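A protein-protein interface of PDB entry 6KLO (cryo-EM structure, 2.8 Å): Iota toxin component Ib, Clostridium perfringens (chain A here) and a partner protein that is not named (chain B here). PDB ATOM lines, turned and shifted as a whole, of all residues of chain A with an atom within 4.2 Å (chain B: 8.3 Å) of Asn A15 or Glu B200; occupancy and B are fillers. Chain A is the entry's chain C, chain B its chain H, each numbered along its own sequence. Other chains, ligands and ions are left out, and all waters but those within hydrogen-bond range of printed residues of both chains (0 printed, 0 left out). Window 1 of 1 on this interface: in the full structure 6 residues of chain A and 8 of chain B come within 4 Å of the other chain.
The side-chain carboxylate (OD2) of Asp A10 lies within hydrogen-bond range of the backbone NH (N) of Asn A15 (2.7 Å).
The backbone carbonyl oxygen (O) of Asn B114 sits close to the side-chain amide oxygen (OD1) of Asn B116 (3.4 Å).
O of Asn B114 is in hydrogen-bond range of NZ of Lys B202 (3.3 Å).
The side-chain amino group (NZ) of Lys B202 is in hydrogen-bond range of the side-chain amide oxygen (OD1) of Asn B116 (2.8 Å).
The backbone NH (N) of Gln B203 sits at hydrogen-bond distance from the backbone carbonyl oxygen (O) of Asn B116, at 2.9 Å.
The side-chain amide oxygen (OD1) of Asn B150 sits close to the side-chain carboxylate (OE1) of Glu B200, at 2.7 Å.
Of the 8 printed residues of chain A, 3 touch a printed residue of chain B.
Printed residues of chain A that touch a printed residue of chain B: Asn A15, Tyr A64 and Gln A65.
Printed residues of chain B that touch a printed residue of chain A: Asn B116, Asn B150, Glu B200, Gly B201 and Lys B202.
Among the printed residues, 7 pairs touch across the chains.
O of Asn A15 is in hydrogen-bond range of ND2 of Asn B116 (3.0 Å).
The backbone NH (N) of Gly B201 lies close to the side-chain hydroxyl (OH) of Tyr A64 (3.4 Å).
The backbone carbonyl oxygen (O) of Glu B200 lies close to the side-chain amide nitrogen (ND2) of Asn A15 (2.3 Å).
Among the printed residues, pairs that only touch across the chains: Asn A15 with Lys B202 (3.2 Å), Tyr A64 with Glu B200 (3.5 Å), Gln A65 with Asn B150 (3.8 Å) and Gln A65 with Glu B200 (3.9 Å).
Asn A15 touches just these residues of chain B: Asn B116, Glu B200 and Lys B202.
Printed residues of chain B within 4 Å of Tyr A64: Glu B200 (3.5 Å) and Gly B201 (3.3 Å).
Of the printed residues of chain A, Asn B116 touches Asn A15 (3.0 Å).
Of the printed residues of chain A, Asn B150 touches Gln A65.
Glu B200 touches just these residues of chain A: Asn A15 (2.3 Å), Tyr A64 (3.5 Å) and Gln A65 (3.9 Å).
Of the printed residues of chain A, Gly B201 touches Tyr A64 (3.3 Å).
Printed residues of chain A within 4 Å of Lys B202: Asn A15.
The nearest residue of chain B that does not touch Asn A15 is Gly B201 (4.2 Å).
The nearest residue of chain A that does not touch Glu B200 is Thr A62 (4.1 Å).
The nearest printed residue of chain A that does not touch Gly B201 is Asn A15 (4.2 Å).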
ATOM      1  N   ASP A  10     -30.695 -24.013  19.484  1.00  0.00           N
ATOM      2  CA  ASP A  10     -30.304 -22.711  20.020  1.00  0.00           C
ATOM      3  C   ASP A  10     -29.736 -21.872  18.882  1.00  0.00           C
ATOM      4  O   ASP A  10     -28.547 -21.969  18.564  1.00  0.00           O
ATOM      5  CB  ASP A  10     -29.288 -22.882  21.144  1.00  0.00           C
ATOM      6  CG  ASP A  10     -29.150 -21.647  21.997  1.00  0.00           C
ATOM      7  OD1 ASP A  10     -30.040 -20.778  21.942  1.00  0.00           O
ATOM      8  OD2 ASP A  10     -28.151 -21.546  22.732  1.00  0.00           O
ATOM      9  N   ASN A  13     -27.535 -18.834  20.175  1.00  0.00           N
ATOM     10  CA  ASN A  13     -26.403 -19.340  20.949  1.00  0.00           C
ATOM     11  C   ASN A  13     -26.265 -18.603  22.282  1.00  0.00           C
ATOM     12  O   ASN A  13     -25.234 -18.007  22.591  1.00  0.00           O
ATOM     13  CB  ASN A  13     -25.103 -19.256  20.143  1.00  0.00           C
ATOM     14  CG  ASN A  13     -24.926 -20.423  19.202  1.00  0.00           C
ATOM     15  OD1 ASN A  13     -24.748 -21.560  19.633  1.00  0.00           O
ATOM     16  ND2 ASN A  13     -24.964 -20.148  17.906  1.00  0.00           N
ATOM     17  N   ASP A  14     -27.334 -18.653  23.076  1.00  0.00           N
ATOM     18  CA  ASP A  14     -27.318 -18.103  24.425  1.00  0.00           C
ATOM     19  C   ASP A  14     -27.763 -19.132  25.458  1.00  0.00           C
ATOM     20  O   ASP A  14     -28.170 -18.762  26.560  1.00  0.00           O
ATOM     21  CB  ASP A  14     -28.182 -16.843  24.513  1.00  0.00           C
ATOM     22  CG  ASP A  14     -29.639 -17.111  24.232  1.00  0.00           C
ATOM     23  OD1 ASP A  14     -29.951 -18.115  23.565  1.00  0.00           O
ATOM     24  OD2 ASP A  14     -30.480 -16.311  24.679  1.00  0.00           O
ATOM     25  N   ASN A  15     -27.707 -20.414  25.107  1.00  0.00           N
ATOM     26  CA  ASN A  15     -27.954 -21.529  26.018  1.00  0.00           C
ATOM     27  C   ASN A  15     -29.392 -21.582  26.515  1.00  0.00           C
ATOM     28  O   ASN A  15     -29.667 -22.185  27.554  1.00  0.00           O
ATOM     29  CB  ASN A  15     -26.982 -21.503  27.199  1.00  0.00           C
ATOM     30  CG  ASN A  15     -25.542 -21.614  26.757  1.00  0.00           C
ATOM     31  OD1 ASN A  15     -25.234 -22.294  25.780  1.00  0.00           O
ATOM     32  ND2 ASN A  15     -24.653 -20.939  27.467  1.00  0.00           N
ATOM     33  N   ILE A  16     -30.320 -20.966  25.794  1.00  0.00           N
ATOM     34  CA  ILE A  16     -31.748 -21.135  26.020  1.00  0.00           C
ATOM     35  C   ILE A  16     -32.356 -21.603  24.704  1.00  0.00           C
ATOM     36  O   ILE A  16     -32.206 -20.929  23.684  1.00  0.00           O
ATOM     37  CB  ILE A  16     -32.425 -19.841  26.502  1.00  0.00           C
ATOM     38  CG1 ILE A  16     -31.609 -19.192  27.614  1.00  0.00           C
ATOM     39  CG2 ILE A  16     -33.819 -20.132  27.011  1.00  0.00           C
ATOM     40  CD1 ILE A  16     -32.236 -17.946  28.159  1.00  0.00           C
ATOM     41  N   THR A  62     -26.763 -10.700  28.264  1.00  0.00           N
ATOM     42  CA  THR A  62     -27.546 -11.612  27.446  1.00  0.00           C
ATOM     43  C   THR A  62     -28.836 -12.003  28.162  1.00  0.00           C
ATOM     44  O   THR A  62     -29.067 -11.660  29.322  1.00  0.00           O
ATOM     45  CB  THR A  62     -26.741 -12.863  27.094  1.00  0.00           C
ATOM     46  OG1 THR A  62     -26.469 -13.612  28.280  1.00  0.00           O
ATOM     47  CG2 THR A  62     -25.433 -12.494  26.433  1.00  0.00           C
ATOM     48  N   TYR A  64     -29.738 -15.049  29.006  1.00  0.00           N
ATOM     49  CA  TYR A  64     -29.463 -16.012  30.062  1.00  0.00           C
ATOM     50  C   TYR A  64     -28.851 -15.339  31.283  1.00  0.00           C
ATOM     51  O   TYR A  64     -29.197 -15.680  32.418  1.00  0.00           O
ATOM     52  CB  TYR A  64     -28.538 -17.117  29.561  1.00  0.00           C
ATOM     53  CG  TYR A  64     -28.121 -18.033  30.679  1.00  0.00           C
ATOM     54  CD1 TYR A  64     -28.977 -19.017  31.141  1.00  0.00           C
ATOM     55  CD2 TYR A  64     -26.892 -17.893  31.299  1.00  0.00           C
ATOM     56  CE1 TYR A  64     -28.618 -19.841  32.173  1.00  0.00           C
ATOM     57  CE2 TYR A  64     -26.524 -18.714  32.334  1.00  0.00           C
ATOM     58  CZ  TYR A  64     -27.392 -19.686  32.767  1.00  0.00           C
ATOM     59  OH  TYR A  64     -27.030 -20.516  33.799  1.00  0.00           O
ATOM     60  N   GLN A  65     -27.924 -14.402  31.074  1.00  0.00           N
ATOM     61  CA  GLN A  65     -27.306 -13.710  32.199  1.00  0.00           C
ATOM     62  C   GLN A  65     -28.346 -12.985  33.034  1.00  0.00           C
ATOM     63  O   GLN A  65     -28.314 -13.043  34.266  1.00  0.00           O
ATOM     64  CB  GLN A  65     -26.254 -12.723  31.703  1.00  0.00           C
ATOM     65  CG  GLN A  65     -24.943 -13.349  31.298  1.00  0.00           C
ATOM     66  CD  GLN A  65     -24.023 -12.357  30.627  1.00  0.00           C
ATOM     67  OE1 GLN A  65     -24.460 -11.311  30.158  1.00  0.00           O
ATOM     68  NE2 GLN A  65     -22.743 -12.679  30.577  1.00  0.00           N
ATOM     69  N   ARG B 111     -23.344 -35.662  25.609  1.00  0.00           N
ATOM     70  CA  ARG B 111     -24.555 -34.899  25.359  1.00  0.00           C
ATOM     71  C   ARG B 111     -24.373 -34.139  24.058  1.00  0.00           C
ATOM     72  O   ARG B 111     -23.267 -33.692  23.746  1.00  0.00           O
ATOM     73  CB  ARG B 111     -24.871 -33.930  26.503  1.00  0.00           C
ATOM     74  CG  ARG B 111     -23.779 -32.919  26.789  1.00  0.00           C
ATOM     75  CD  ARG B 111     -24.371 -31.547  27.044  1.00  0.00           C
ATOM     76  NE  ARG B 111     -23.368 -30.597  27.505  1.00  0.00           N
ATOM     77  CZ  ARG B 111     -22.578 -29.896  26.701  1.00  0.00           C
ATOM     78  NH1 ARG B 111     -22.674 -30.035  25.388  1.00  0.00           N
ATOM     79  NH2 ARG B 111     -21.694 -29.051  27.209  1.00  0.00           N
ATOM     80  N   GLU B 113     -24.213 -31.277  21.351  1.00  0.00           N
ATOM     81  CA  GLU B 113     -23.659 -29.938  21.523  1.00  0.00           C
ATOM     82  C   GLU B 113     -24.729 -28.883  21.753  1.00  0.00           C
ATOM     83  O   GLU B 113     -24.400 -27.787  22.219  1.00  0.00           O
ATOM     84  CB  GLU B 113     -22.812 -29.559  20.307  1.00  0.00           C
ATOM     85  CG  GLU B 113     -21.594 -30.446  20.085  1.00  0.00           C
ATOM     86  CD  GLU B 113     -20.930 -30.879  21.382  1.00  0.00           C
ATOM     87  OE1 GLU B 113     -20.886 -32.098  21.649  1.00  0.00           O
ATOM     88  OE2 GLU B 113     -20.445 -30.004  22.127  1.00  0.00           O
ATOM     89  N   ASN B 114     -25.994 -29.183  21.452  1.00  0.00           N
ATOM     90  CA  ASN B 114     -27.089 -28.262  21.717  1.00  0.00           C
ATOM     91  C   ASN B 114     -27.761 -28.491  23.061  1.00  0.00           C
ATOM     92  O   ASN B 114     -28.336 -27.548  23.613  1.00  0.00           O
ATOM     93  CB  ASN B 114     -28.146 -28.354  20.612  1.00  0.00           C
ATOM     94  CG  ASN B 114     -27.727 -27.640  19.348  1.00  0.00           C
ATOM     95  OD1 ASN B 114     -27.659 -28.238  18.275  1.00  0.00           O
ATOM     96  ND2 ASN B 114     -27.435 -26.351  19.471  1.00  0.00           N
ATOM     97  N   GLN B 115     -27.709 -29.708  23.596  1.00  0.00           N
ATOM     98  CA  GLN B 115     -28.333 -29.980  24.879  1.00  0.00           C
ATOM     99  C   GLN B 115     -27.599 -29.248  25.997  1.00  0.00           C
ATOM    100  O   GLN B 115     -26.452 -28.819  25.854  1.00  0.00           O
ATOM    101  CB  GLN B 115     -28.354 -31.481  25.156  1.00  0.00           C
ATOM    102  CG  GLN B 115     -29.506 -32.213  24.502  1.00  0.00           C
ATOM    103  CD  GLN B 115     -29.558 -33.671  24.893  1.00  0.00           C
ATOM    104  OE1 GLN B 115     -29.166 -34.042  25.998  1.00  0.00           O
ATOM    105  NE2 GLN B 115     -30.041 -34.509  23.985  1.00  0.00           N
ATOM    106  N   ASN B 116     -28.279 -29.109  27.134  1.00  0.00           N
ATOM    107  CA  ASN B 116     -27.734 -28.400  28.280  1.00  0.00           C
ATOM    108  C   ASN B 116     -27.467 -29.282  29.487  1.00  0.00           C
ATOM    109  O   ASN B 116     -26.641 -28.908  30.324  1.00  0.00           O
ATOM    110  CB  ASN B 116     -28.676 -27.264  28.708  1.00  0.00           C
ATOM    111  CG  ASN B 116     -28.690 -26.119  27.720  1.00  0.00           C
ATOM    112  OD1 ASN B 116     -28.006 -26.158  26.700  1.00  0.00           O
ATOM    113  ND2 ASN B 116     -29.473 -25.092  28.017  1.00  0.00           N
ATOM    114  N   PRO B 148     -11.977 -21.812  31.031  1.00  0.00           N
ATOM    115  CA  PRO B 148     -12.665 -21.083  29.962  1.00  0.00           C
ATOM    116  C   PRO B 148     -13.945 -20.437  30.472  1.00  0.00           C
ATOM    117  O   PRO B 148     -14.715 -21.045  31.217  1.00  0.00           O
ATOM    118  CB  PRO B 148     -12.956 -22.170  28.923  1.00  0.00           C
ATOM    119  CG  PRO B 148     -12.995 -23.429  29.717  1.00  0.00           C
ATOM    120  CD  PRO B 148     -11.968 -23.264  30.792  1.00  0.00           C
ATOM    121  N   GLY B 149     -14.163 -19.192  30.062  1.00  0.00           N
ATOM    122  CA  GLY B 149     -15.335 -18.453  30.485  1.00  0.00           C
ATOM    123  C   GLY B 149     -16.152 -17.920  29.326  1.00  0.00           C
ATOM    124  O   GLY B 149     -16.440 -18.651  28.374  1.00  0.00           O
ATOM    125  N   ASN B 150     -16.529 -16.646  29.395  1.00  0.00           N
ATOM    126  CA  ASN B 150     -17.340 -16.035  28.351  1.00  0.00           C
ATOM    127  C   ASN B 150     -16.478 -15.699  27.141  1.00  0.00           C
ATOM    128  O   ASN B 150     -15.406 -15.100  27.277  1.00  0.00           O
ATOM    129  CB  ASN B 150     -18.073 -14.817  28.912  1.00  0.00           C
ATOM    130  CG  ASN B 150     -19.006 -15.171  30.052  1.00  0.00           C
ATOM    131  OD1 ASN B 150     -19.454 -16.311  30.169  1.00  0.00           O
ATOM    132  ND2 ASN B 150     -19.305 -14.193  30.898  1.00  0.00           N
ATOM    133  N   GLY B 151     -16.948 -16.088  25.957  1.00  0.00           N
ATOM    134  CA  GLY B 151     -16.224 -15.890  24.724  1.00  0.00           C
ATOM    135  C   GLY B 151     -15.266 -17.012  24.376  1.00  0.00           C
ATOM    136  O   GLY B 151     -14.962 -17.212  23.195  1.00  0.00           O
ATOM    137  N   LYS B 154     -15.636 -23.542  23.573  1.00  0.00           N
ATOM    138  CA  LYS B 154     -15.959 -24.727  24.364  1.00  0.00           C
ATOM    139  C   LYS B 154     -16.487 -25.800  23.418  1.00  0.00           C
ATOM    140  O   LYS B 154     -17.705 -26.010  23.315  1.00  0.00           O
ATOM    141  CB  LYS B 154     -16.969 -24.393  25.459  1.00  0.00           C
ATOM    142  CG  LYS B 154     -16.528 -23.242  26.353  1.00  0.00           C
ATOM    143  CD  LYS B 154     -17.492 -23.017  27.502  1.00  0.00           C
ATOM    144  CE  LYS B 154     -18.445 -21.871  27.210  1.00  0.00           C
ATOM    145  NZ  LYS B 154     -17.761 -20.552  27.231  1.00  0.00           N
ATOM    146  N   ILE B 197     -20.142 -29.699  36.101  1.00  0.00           N
ATOM    147  CA  ILE B 197     -19.959 -28.260  36.216  1.00  0.00           C
ATOM    148  C   ILE B 197     -21.038 -27.587  35.383  1.00  0.00           C
ATOM    149  O   ILE B 197     -21.552 -28.172  34.428  1.00  0.00           O
ATOM    150  CB  ILE B 197     -18.552 -27.839  35.733  1.00  0.00           C
ATOM    151  CG1 ILE B 197     -17.483 -28.681  36.419  1.00  0.00           C
ATOM    152  CG2 ILE B 197     -18.295 -26.376  35.990  1.00  0.00           C
ATOM    153  CD1 ILE B 197     -17.421 -28.476  37.904  1.00  0.00           C
ATOM    154  N   VAL B 198     -21.388 -26.357  35.744  1.00  0.00           N
ATOM    155  CA  VAL B 198     -22.290 -25.537  34.942  1.00  0.00           C
ATOM    156  C   VAL B 198     -21.545 -24.274  34.536  1.00  0.00           C
ATOM    157  O   VAL B 198     -21.083 -23.516  35.397  1.00  0.00           O
ATOM    158  CB  VAL B 198     -23.582 -25.190  35.695  1.00  0.00           C
ATOM    159  CG1 VAL B 198     -24.442 -24.277  34.851  1.00  0.00           C
ATOM    160  CG2 VAL B 198     -24.341 -26.450  36.042  1.00  0.00           C
ATOM    161  N   ILE B 199     -21.426 -24.054  33.230  1.00  0.00           N
ATOM    162  CA  ILE B 199     -20.795 -22.862  32.676  1.00  0.00           C
ATOM    163  C   ILE B 199     -21.780 -22.205  31.721  1.00  0.00           C
ATOM    164  O   ILE B 199     -22.183 -22.818  30.725  1.00  0.00           O
ATOM    165  CB  ILE B 199     -19.477 -23.182  31.954  1.00  0.00           C
ATOM    166  CG1 ILE B 199     -18.473 -23.805  32.922  1.00  0.00           C
ATOM    167  CG2 ILE B 199     -18.897 -21.929  31.328  1.00  0.00           C
ATOM    168  CD1 ILE B 199     -17.183 -24.228  32.266  1.00  0.00           C
ATOM    169  N   GLU B 200     -22.185 -20.974  32.039  1.00  0.00           N
ATOM    170  CA  GLU B 200     -23.004 -20.147  31.151  1.00  0.00           C
ATOM    171  C   GLU B 200     -24.295 -20.867  30.757  1.00  0.00           C
ATOM    172  O   GLU B 200     -24.872 -20.622  29.697  1.00  0.00           O
ATOM    173  CB  GLU B 200     -22.192 -19.728  29.918  1.00  0.00           C
ATOM    174  CG  GLU B 200     -22.805 -18.649  29.030  1.00  0.00           C
ATOM    175  CD  GLU B 200     -22.863 -17.291  29.698  1.00  0.00           C
ATOM    176  OE1 GLU B 200     -22.022 -17.029  30.583  1.00  0.00           O
ATOM    177  OE2 GLU B 200     -23.747 -16.485  29.336  1.00  0.00           O
ATOM    178  N   GLY B 201     -24.765 -21.766  31.616  1.00  0.00           N
ATOM    179  CA  GLY B 201     -26.012 -22.455  31.354  1.00  0.00           C
ATOM    180  C   GLY B 201     -25.895 -23.796  30.670  1.00  0.00           C
ATOM    181  O   GLY B 201     -26.917 -24.356  30.268  1.00  0.00           O
ATOM    182  N   LYS B 202     -24.687 -24.332  30.519  1.00  0.00           N
ATOM    183  CA  LYS B 202     -24.498 -25.665  29.966  1.00  0.00           C
ATOM    184  C   LYS B 202     -23.694 -26.504  30.943  1.00  0.00           C
ATOM    185  O   LYS B 202     -22.789 -25.998  31.607  1.00  0.00           O
ATOM    186  CB  LYS B 202     -23.779 -25.631  28.618  1.00  0.00           C
ATOM    187  CG  LYS B 202     -24.539 -24.939  27.515  1.00  0.00           C
ATOM    188  CD  LYS B 202     -23.850 -25.140  26.175  1.00  0.00           C
ATOM    189  CE  LYS B 202     -24.189 -26.491  25.587  1.00  0.00           C
ATOM    190  NZ  LYS B 202     -25.646 -26.622  25.338  1.00  0.00           N
ATOM    191  N   GLN B 203     -24.016 -27.789  31.019  1.00  0.00           N
ATOM    192  CA  GLN B 203     -23.320 -28.691  31.920  1.00  0.00           C
ATOM    193  C   GLN B 203     -22.148 -29.354  31.212  1.00  0.00           C
ATOM    194  O   GLN B 203     -22.266 -29.807  30.070  1.00  0.00           O
ATOM    195  CB  GLN B 203     -24.280 -29.744  32.471  1.00  0.00           C
ATOM    196  CG  GLN B 203     -25.354 -29.160  33.366  1.00  0.00           C
ATOM    197  CD  GLN B 203     -26.161 -30.214  34.086  1.00  0.00           C
ATOM    198  OE1 GLN B 203     -25.608 -31.095  34.744  1.00  0.00           O
ATOM    199  NE2 GLN B 203     -27.478 -30.124  33.979  1.00  0.00           N
ATOM    200  N   TYR B 204     -21.013 -29.401  31.903  1.00  0.00           N
ATOM    201  CA  TYR B 204     -19.781 -29.997  31.411  1.00  0.00           C
ATOM    202  C   TYR B 204     -19.265 -30.993  32.439  1.00  0.00           C
ATOM    203  O   TYR B 204     -19.742 -31.052  33.573  1.00  0.00           O
ATOM    204  CB  TYR B 204     -18.707 -28.936  31.141  1.00  0.00           C
ATOM    205  CG  TYR B 204     -19.051 -27.939  30.062  1.00  0.00           C
ATOM    206  CD1 TYR B 204     -19.816 -26.819  30.345  1.00  0.00           C
ATOM    207  CD2 TYR B 204     -18.593 -28.106  28.767  1.00  0.00           C
ATOM    208  CE1 TYR B 204     -20.124 -25.902  29.364  1.00  0.00           C
ATOM    209  CE2 TYR B 204     -18.897 -27.195  27.780  1.00  0.00           C
ATOM    210  CZ  TYR B 204     -19.661 -26.095  28.084  1.00  0.00           C
ATOM    211  OH  TYR B 204     -19.966 -25.182  27.103  1.00  0.00           O
